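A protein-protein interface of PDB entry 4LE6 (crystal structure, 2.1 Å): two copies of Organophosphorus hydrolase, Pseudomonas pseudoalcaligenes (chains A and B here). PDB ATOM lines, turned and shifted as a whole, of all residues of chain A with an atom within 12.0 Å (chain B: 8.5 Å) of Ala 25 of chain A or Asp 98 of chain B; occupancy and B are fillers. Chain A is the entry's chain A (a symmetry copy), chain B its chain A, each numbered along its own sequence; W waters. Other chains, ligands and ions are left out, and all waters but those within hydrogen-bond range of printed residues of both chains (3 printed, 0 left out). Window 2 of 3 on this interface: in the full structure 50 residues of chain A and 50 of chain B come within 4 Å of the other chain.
The backbone carbonyl oxygen (O) of Asp 44 of chain B sits at hydrogen-bond distance from the side-chain amide nitrogen (NE2) of Gln 29 of chain A, at 2.8 Å.
O of Pro 27 of chain A lies within hydrogen-bond range of ND2 of Asn 95 of chain B (2.9 Å).
The backbone NH (N) of Ala 25 of chain A sits at hydrogen-bond distance from the backbone carbonyl oxygen (O) of Gly 97 of chain B.
The backbone NH (N) of Ala 26 of chain A sits at hydrogen-bond distance from the backbone carbonyl oxygen (O) of Gly 97 of chain B (3.0 Å).
Of chain B, only Gly 97 and Asp 98 come within 4 Å of Ala 25 of chain A.
Printed residues of chain B within 4 Å of Pro 27 of chain A: Asn 95 and Gln 131.
Printed residues of chain B within 4 Å of Ala 28 of chain A: Asn 95.
Lys 31 of chain A touches none of the printed residues of chain B.
Printed residues of chain A within 4 Å of Phe 45 of chain B: Gln 29.
Asn 95 of chain B touches four residues of chain A.
No residue of chain A comes within 4 Å of Thr 96 of chain B.
Of chain A, only Ala 25 (3.1 Å) and Ala 26 (3.0 Å) come within 4 Å of Gly 97 of chain B.
Asp 98 of chain B touches two residues of chain A.
Asn 99 of chain B touches one residue of chain A.
Of the printed residues of chain A, Leu 100 of chain B touches Ala 26 (3.9 Å).
Gly 217 of chain B touches none of the printed residues of chain A.
The nearest printed residue of chain B that does not touch Ala 28 of chain A is Gln 131 of chain B (6.4 Å).
Among the printed residues, merely in contact across the chains: Ala 26 of chain A with Asn 95 of chain B, Pro 27 of chain A with Gln 131 of chain B, Gln 29 of chain A with Asn 95 of chain B, Ala 26 of chain A with Asn 99 of chain B, Ala 26 of chain A with Asp 98 of chain B, Ala 28 of chain A with Asn 95 of chain B, Ala 25 of chain A with Asp 98 of chain B, Ala 26 of chain A with Leu 100 of chain B and Gln 29 of chain A with Phe 45 of chain B.
Hydrophobic or aromatic side chains of chain A within 4 Å of the printed part of chain B: Ala 25, Ala 26 and Pro 27.
No position is printed for both chains.
OG1 of Thr 96 of chain B lies close to N of Asp 98 of chain B, 3.2 Å away.
OG1 of Thr 96 of chain B lies within hydrogen-bond range of N of Asn 99 of chain B, 2.8 Å away.
ND2 of Asn 99 of chain B is in hydrogen-bond range of OD1 of Asp 133 of chain B (2.9 Å).
The backbone NH of Leu 100 of chain B is in hydrogen-bond range of the side-chain carboxylate of Asp 133 of chain B, 2.7 Å away.
O of Leu 100 of chain B lies within hydrogen-bond range of N of Thr 134 of chain B, 3.4 Å away.
The side-chain amino group (NZ) of Lys 31 of chain A lies within hydrogen-bond range of the side-chain amide oxygen (OE1) of Gln 29 of chain A.
Water W1 bridges OD2 of Asp 133 of chain B (2.6 Å) and O of Ala 25 of chain A (3.4 Å).
Water W2 bridges the backbone carbonyl oxygen (O) of Pro 27 of chain A (2.9 Å) and the side-chain amide oxygen (OD1) of Asn 95 of chain B (2.9 Å).
Water W3 lies within hydrogen-bond range of the backbone carbonyl oxygen (O) of Asp 44 of chain B (3.2 Å) and the side-chain amide nitrogen (NE2) of Gln 29 of chain A (3.3 Å).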
ATOM      1  N   ALA A  25     -16.902  12.173  18.182  1.00  0.00           N
ATOM      2  CA  ALA A  25     -16.256  10.946  17.746  1.00  0.00           C
ATOM      3  C   ALA A  25     -14.813  10.881  18.228  1.00  0.00           C
ATOM      4  O   ALA A  25     -14.183   9.833  18.125  1.00  0.00           O
ATOM      5  CB  ALA A  25     -16.310  10.818  16.247  1.00  0.00           C
ATOM      6  N   ALA A  26     -14.291  11.985  18.764  1.00  0.00           N
ATOM      7  CA  ALA A  26     -12.998  11.947  19.400  1.00  0.00           C
ATOM      8  C   ALA A  26     -13.170  11.087  20.639  1.00  0.00           C
ATOM      9  O   ALA A  26     -14.279  10.978  21.149  1.00  0.00           O
ATOM     10  CB  ALA A  26     -12.538  13.360  19.800  1.00  0.00           C
ATOM     11  N   PRO A  27     -12.082  10.485  21.138  1.00  0.00           N
ATOM     12  CA  PRO A  27     -12.146   9.831  22.448  1.00  0.00           C
ATOM     13  C   PRO A  27     -12.466  10.856  23.529  1.00  0.00           C
ATOM     14  O   PRO A  27     -12.350  12.059  23.305  1.00  0.00           O
ATOM     15  CB  PRO A  27     -10.715   9.327  22.674  1.00  0.00           C
ATOM     16  CG  PRO A  27     -10.053   9.361  21.349  1.00  0.00           C
ATOM     17  CD  PRO A  27     -10.727  10.455  20.573  1.00  0.00           C
ATOM     18  N   ALA A  28     -12.833  10.373  24.703  1.00  0.00           N
ATOM     19  CA  ALA A  28     -13.074  11.235  25.830  1.00  0.00           C
ATOM     20  C   ALA A  28     -11.806  12.028  26.125  1.00  0.00           C
ATOM     21  O   ALA A  28     -10.689  11.541  25.910  1.00  0.00           O
ATOM     22  CB  ALA A  28     -13.484  10.394  27.039  1.00  0.00           C
ATOM     23  N   GLN A  29     -11.969  13.256  26.599  1.00  0.00           N
ATOM     24  CA  GLN A  29     -10.832  14.079  26.967  1.00  0.00           C
ATOM     25  C   GLN A  29     -10.170  13.506  28.204  1.00  0.00           C
ATOM     26  O   GLN A  29     -10.840  13.037  29.117  1.00  0.00           O
ATOM     27  CB  GLN A  29     -11.279  15.513  27.232  1.00  0.00           C
ATOM     28  CG  GLN A  29     -11.639  16.264  25.936  1.00  0.00           C
ATOM     29  CD  GLN A  29     -12.228  17.643  26.184  1.00  0.00           C
ATOM     30  OE1 GLN A  29     -12.316  18.096  27.322  1.00  0.00           O
ATOM     31  NE2 GLN A  29     -12.637  18.314  25.116  1.00  0.00           N
ATOM     32  N   GLN A  30      -8.850  13.557  28.238  1.00  0.00           N
ATOM     33  CA  GLN A  30      -8.097  12.988  29.349  1.00  0.00           C
ATOM     34  C   GLN A  30      -8.157  13.843  30.610  1.00  0.00           C
ATOM     35  O   GLN A  30      -8.173  13.303  31.722  1.00  0.00           O
ATOM     36  CB  GLN A  30      -6.659  12.743  28.916  1.00  0.00           C
ATOM     37  CG  GLN A  30      -6.546  11.518  28.019  1.00  0.00           C
ATOM     38  CD  GLN A  30      -6.626  10.228  28.802  1.00  0.00           C
ATOM     39  OE1 GLN A  30      -5.931  10.070  29.798  1.00  0.00           O
ATOM     40  NE2 GLN A  30      -7.471   9.296  28.357  1.00  0.00           N
ATOM     41  N   LYS A  31      -8.234  15.163  30.435  1.00  0.00           N
ATOM     42  CA  LYS A  31      -8.338  16.107  31.554  1.00  0.00           C
ATOM     43  C   LYS A  31      -7.012  16.227  32.314  1.00  0.00           C
ATOM     44  O   LYS A  31      -6.432  17.312  32.418  1.00  0.00           O
ATOM     45  CB  LYS A  31      -9.470  15.714  32.515  1.00  0.00           C
ATOM     46  CG  LYS A  31     -10.587  16.730  32.600  1.00  0.00           C
ATOM     47  CD  LYS A  31     -11.485  16.659  31.379  1.00  0.00           C
ATOM     48  CE  LYS A  31     -12.371  17.889  31.278  1.00  0.00           C
ATOM     49  NZ  LYS A  31     -13.126  17.920  29.999  1.00  0.00           N
ATOM     50  N   ASP B  44     -14.247  24.353  25.007  1.00  0.00           N
ATOM     51  CA  ASP B  44     -14.601  22.945  25.154  1.00  0.00           C
ATOM     52  C   ASP B  44     -13.544  22.039  24.531  1.00  0.00           C
ATOM     53  O   ASP B  44     -13.670  20.824  24.571  1.00  0.00           O
ATOM     54  CB  ASP B  44     -15.959  22.660  24.510  1.00  0.00           C
ATOM     55  CG  ASP B  44     -17.083  23.397  25.185  1.00  0.00           C
ATOM     56  OD1 ASP B  44     -17.023  23.545  26.421  1.00  0.00           O
ATOM     57  OD2 ASP B  44     -18.017  23.837  24.477  1.00  0.00           O
ATOM     58  N   PHE B  45     -12.498  22.618  23.954  1.00  0.00           N
ATOM     59  CA  PHE B  45     -11.421  21.799  23.408  1.00  0.00           C
ATOM     60  C   PHE B  45     -10.384  21.489  24.478  1.00  0.00           C
ATOM     61  O   PHE B  45     -10.237  22.227  25.467  1.00  0.00           O
ATOM     62  CB  PHE B  45     -10.715  22.492  22.249  1.00  0.00           C
ATOM     63  CG  PHE B  45     -11.587  22.737  21.046  1.00  0.00           C
ATOM     64  CD1 PHE B  45     -12.899  22.274  20.986  1.00  0.00           C
ATOM     65  CD2 PHE B  45     -11.082  23.422  19.958  1.00  0.00           C
ATOM     66  CE1 PHE B  45     -13.677  22.502  19.860  1.00  0.00           C
ATOM     67  CE2 PHE B  45     -11.864  23.660  18.842  1.00  0.00           C
ATOM     68  CZ  PHE B  45     -13.159  23.203  18.795  1.00  0.00           C
ATOM     69  N   ILE B  94      -4.992  18.312  19.676  1.00  0.00           N
ATOM     70  CA  ILE B  94      -6.184  19.004  20.126  1.00  0.00           C
ATOM     71  C   ILE B  94      -7.382  18.079  19.973  1.00  0.00           C
ATOM     72  O   ILE B  94      -7.651  17.546  18.889  1.00  0.00           O
ATOM     73  CB  ILE B  94      -6.378  20.322  19.363  1.00  0.00           C
ATOM     74  CG1 ILE B  94      -5.158  21.223  19.612  1.00  0.00           C
ATOM     75  CG2 ILE B  94      -7.638  21.044  19.828  1.00  0.00           C
ATOM     76  CD1 ILE B  94      -5.149  22.496  18.835  1.00  0.00           C
ATOM     77  N   ASN B  95      -8.062  17.857  21.091  1.00  0.00           N
ATOM     78  CA  ASN B  95      -9.277  17.048  21.122  1.00  0.00           C
ATOM     79  C   ASN B  95     -10.440  18.036  21.116  1.00  0.00           C
ATOM     80  O   ASN B  95     -10.668  18.747  22.106  1.00  0.00           O
ATOM     81  CB  ASN B  95      -9.291  16.178  22.391  1.00  0.00           C
ATOM     82  CG  ASN B  95     -10.505  15.266  22.471  1.00  0.00           C
ATOM     83  OD1 ASN B  95     -11.574  15.614  21.984  1.00  0.00           O
ATOM     84  ND2 ASN B  95     -10.348  14.096  23.096  1.00  0.00           N
ATOM     85  N   THR B  96     -11.136  18.119  19.981  1.00  0.00           N
ATOM     86  CA  THR B  96     -12.196  19.092  19.787  1.00  0.00           C
ATOM     87  C   THR B  96     -13.568  18.501  20.105  1.00  0.00           C
ATOM     88  O   THR B  96     -14.587  19.139  19.858  1.00  0.00           O
ATOM     89  CB  THR B  96     -12.269  19.551  18.317  1.00  0.00           C
ATOM     90  OG1 THR B  96     -12.697  18.456  17.489  1.00  0.00           O
ATOM     91  CG2 THR B  96     -10.940  20.036  17.844  1.00  0.00           C
ATOM     92  N   GLY B  97     -13.591  17.282  20.634  1.00  0.00           N
ATOM     93  CA  GLY B  97     -14.837  16.538  20.749  1.00  0.00           C
ATOM     94  C   GLY B  97     -15.227  15.861  19.434  1.00  0.00           C
ATOM     95  O   GLY B  97     -15.522  14.664  19.408  1.00  0.00           O
ATOM     96  N   ASP B  98     -15.224  16.616  18.339  1.00  0.00           N
ATOM     97  CA  ASP B  98     -15.537  16.057  17.030  1.00  0.00           C
ATOM     98  C   ASP B  98     -14.369  15.282  16.441  1.00  0.00           C
ATOM     99  O   ASP B  98     -14.563  14.299  15.744  1.00  0.00           O
ATOM    100  CB  ASP B  98     -15.936  17.161  16.042  1.00  0.00           C
ATOM    101  CG  ASP B  98     -17.240  17.825  16.410  1.00  0.00           C
ATOM    102  OD1 ASP B  98     -18.285  17.150  16.336  1.00  0.00           O
ATOM    103  OD2 ASP B  98     -17.219  19.018  16.780  1.00  0.00           O
ATOM    104  N   ASN B  99     -13.160  15.767  16.686  1.00  0.00           N
ATOM    105  CA  ASN B  99     -11.955  15.175  16.129  1.00  0.00           C
ATOM    106  C   ASN B  99     -10.805  15.147  17.129  1.00  0.00           C
ATOM    107  O   ASN B  99     -10.696  16.017  18.006  1.00  0.00           O
ATOM    108  CB  ASN B  99     -11.490  15.977  14.916  1.00  0.00           C
ATOM    109  CG  ASN B  99     -12.514  16.000  13.799  1.00  0.00           C
ATOM    110  OD1 ASN B  99     -13.347  16.910  13.719  1.00  0.00           O
ATOM    111  ND2 ASN B  99     -12.461  14.997  12.928  1.00  0.00           N
ATOM    112  N   LEU B 100      -9.924  14.166  16.975  1.00  0.00           N
ATOM    113  CA  LEU B 100      -8.626  14.219  17.632  1.00  0.00           C
ATOM    114  C   LEU B 100      -7.618  14.595  16.558  1.00  0.00           C
ATOM    115  O   LEU B 100      -7.392  13.843  15.605  1.00  0.00           O
ATOM    116  CB  LEU B 100      -8.264  12.894  18.300  1.00  0.00           C
ATOM    117  CG  LEU B 100      -6.970  12.928  19.124  1.00  0.00           C
ATOM    118  CD1 LEU B 100      -7.087  13.832  20.366  1.00  0.00           C
ATOM    119  CD2 LEU B 100      -6.588  11.530  19.536  1.00  0.00           C
ATOM    120  N   VAL B 101      -7.032  15.778  16.711  1.00  0.00           N
ATOM    121  CA  VAL B 101      -6.235  16.384  15.658  1.00  0.00           C
ATOM    122  C   VAL B 101      -4.816  16.614  16.132  1.00  0.00           C
ATOM    123  O   VAL B 101      -4.590  17.262  17.152  1.00  0.00           O
ATOM    124  CB  VAL B 101      -6.831  17.756  15.227  1.00  0.00           C
ATOM    125  CG1 VAL B 101      -6.017  18.362  14.087  1.00  0.00           C
ATOM    126  CG2 VAL B 101      -8.279  17.601  14.810  1.00  0.00           C
ATOM    127  N   GLN B 131      -5.687   6.610  17.566  1.00  0.00           N
ATOM    128  CA  GLN B 131      -6.860   7.464  17.803  1.00  0.00           C
ATOM    129  C   GLN B 131      -6.838   8.767  16.999  1.00  0.00           C
ATOM    130  O   GLN B 131      -7.855   9.460  16.888  1.00  0.00           O
ATOM    131  CB  GLN B 131      -6.978   7.812  19.294  1.00  0.00           C
ATOM    132  CG  GLN B 131      -7.238   6.607  20.210  1.00  0.00           C
ATOM    133  CD  GLN B 131      -7.199   6.985  21.692  1.00  0.00           C
ATOM    134  OE1 GLN B 131      -6.284   7.670  22.140  1.00  0.00           O
ATOM    135  NE2 GLN B 131      -8.213   6.586  22.435  1.00  0.00           N
ATOM    136  N   ASP B 133      -7.321  11.036  14.174  1.00  0.00           N
ATOM    137  CA  ASP B 133      -8.085  10.933  12.924  1.00  0.00           C
ATOM    138  C   ASP B 133      -7.659  11.978  11.888  1.00  0.00           C
ATOM    139  O   ASP B 133      -7.964  11.852  10.705  1.00  0.00           O
ATOM    140  CB  ASP B 133      -9.601  11.034  13.183  1.00  0.00           C
ATOM    141  CG  ASP B 133     -10.020  12.416  13.667  1.00  0.00           C
ATOM    142  OD1 ASP B 133     -10.081  13.353  12.845  1.00  0.00           O
ATOM    143  OD2 ASP B 133     -10.293  12.575  14.871  1.00  0.00           O
ATOM    144  N   THR B 134      -6.933  12.996  12.325  1.00  0.00           N
ATOM    145  CA  THR B 134      -6.435  14.027  11.427  1.00  0.00           C
ATOM    146  C   THR B 134      -5.040  14.467  11.861  1.00  0.00           C
ATOM    147  O   THR B 134      -4.797  14.661  13.053  1.00  0.00           O
ATOM    148  CB  THR B 134      -7.313  15.286  11.452  1.00  0.00           C
ATOM    149  OG1 THR B 134      -8.679  14.939  11.221  1.00  0.00           O
ATOM    150  CG2 THR B 134      -6.865  16.269  10.379  1.00  0.00           C
ATOM    151  N   GLU B 211     -18.444  22.134  10.434  1.00  0.00           N
ATOM    152  CA  GLU B 211     -18.390  23.528  10.858  1.00  0.00           C
ATOM    153  C   GLU B 211     -16.971  24.074  10.672  1.00  0.00           C
ATOM    154  O   GLU B 211     -16.200  23.522   9.885  1.00  0.00           O
ATOM    155  CB  GLU B 211     -18.837  23.657  12.316  1.00  0.00           C
ATOM    156  CG  GLU B 211     -20.183  23.003  12.612  1.00  0.00           C
ATOM    157  CD  GLU B 211     -20.600  23.147  14.065  1.00  0.00           C
ATOM    158  OE1 GLU B 211     -19.739  23.488  14.904  1.00  0.00           O
ATOM    159  OE2 GLU B 211     -21.791  22.919  14.368  1.00  0.00           O
ATOM    160  N   GLY B 212     -16.629  25.138  11.402  1.00  0.00           N
ATOM    161  CA  GLY B 212     -15.327  25.781  11.287  1.00  0.00           C
ATOM    162  C   GLY B 212     -15.009  26.102   9.836  1.00  0.00           C
ATOM    163  O   GLY B 212     -15.483  27.105   9.298  1.00  0.00           O
ATOM    164  N   LEU B 215     -12.349  21.708   9.508  1.00  0.00           N
ATOM    165  CA  LEU B 215     -13.069  20.843  10.435  1.00  0.00           C
ATOM    166  C   LEU B 215     -13.841  21.754  11.371  1.00  0.00           C
ATOM    167  O   LEU B 215     -13.576  22.951  11.412  1.00  0.00           O
ATOM    168  CB  LEU B 215     -12.105  19.997  11.250  1.00  0.00           C
ATOM    169  CG  LEU B 215     -11.323  18.916  10.516  1.00  0.00           C
ATOM    170  CD1 LEU B 215     -10.289  18.390  11.469  1.00  0.00           C
ATOM    171  CD2 LEU B 215     -12.264  17.792  10.020  1.00  0.00           C
ATOM    172  N   PRO B 216     -14.802  21.205  12.124  1.00  0.00           N
ATOM    173  CA  PRO B 216     -15.505  22.073  13.079  1.00  0.00           C
ATOM    174  C   PRO B 216     -14.511  22.742  14.041  1.00  0.00           C
ATOM    175  O   PRO B 216     -13.742  22.034  14.681  1.00  0.00           O
ATOM    176  CB  PRO B 216     -16.434  21.101  13.823  1.00  0.00           C
ATOM    177  CG  PRO B 216     -16.660  19.967  12.837  1.00  0.00           C
ATOM    178  CD  PRO B 216     -15.337  19.829  12.119  1.00  0.00           C
ATOM    179  N   GLY B 217     -14.493  24.070  14.076  1.00  0.00           N
ATOM    180  CA  GLY B 217     -13.653  24.811  14.997  1.00  0.00           C
ATOM    181  C   GLY B 217     -12.244  25.031  14.481  1.00  0.00           C
ATOM    182  O   GLY B 217     -11.435  25.683  15.127  1.00  0.00           O
ATOM    183  N   VAL B 218     -11.957  24.500  13.301  1.00  0.00           N
ATOM    184  CA  VAL B 218     -10.592  24.506  12.771  1.00  0.00           C
ATOM    185  C   VAL B 218     -10.543  25.161  11.400  1.00  0.00           C
ATOM    186  O   VAL B 218     -11.284  24.784  10.496  1.00  0.00           O
ATOM    187  CB  VAL B 218     -10.020  23.095  12.661  1.00  0.00           C
ATOM    188  CG1 VAL B 218      -8.528  23.167  12.364  1.00  0.00           C
ATOM    189  CG2 VAL B 218     -10.258  22.332  13.959  1.00  0.00           C
HETATM  190  O   HOH W   1     -11.689  10.749  16.011  1.00  0.00           O
HETATM  191  O   HOH W   2     -13.883  14.502  23.364  1.00  0.00           O
HETATM  192  O   HOH W   3     -15.745  18.487  23.907  1.00  0.00           O
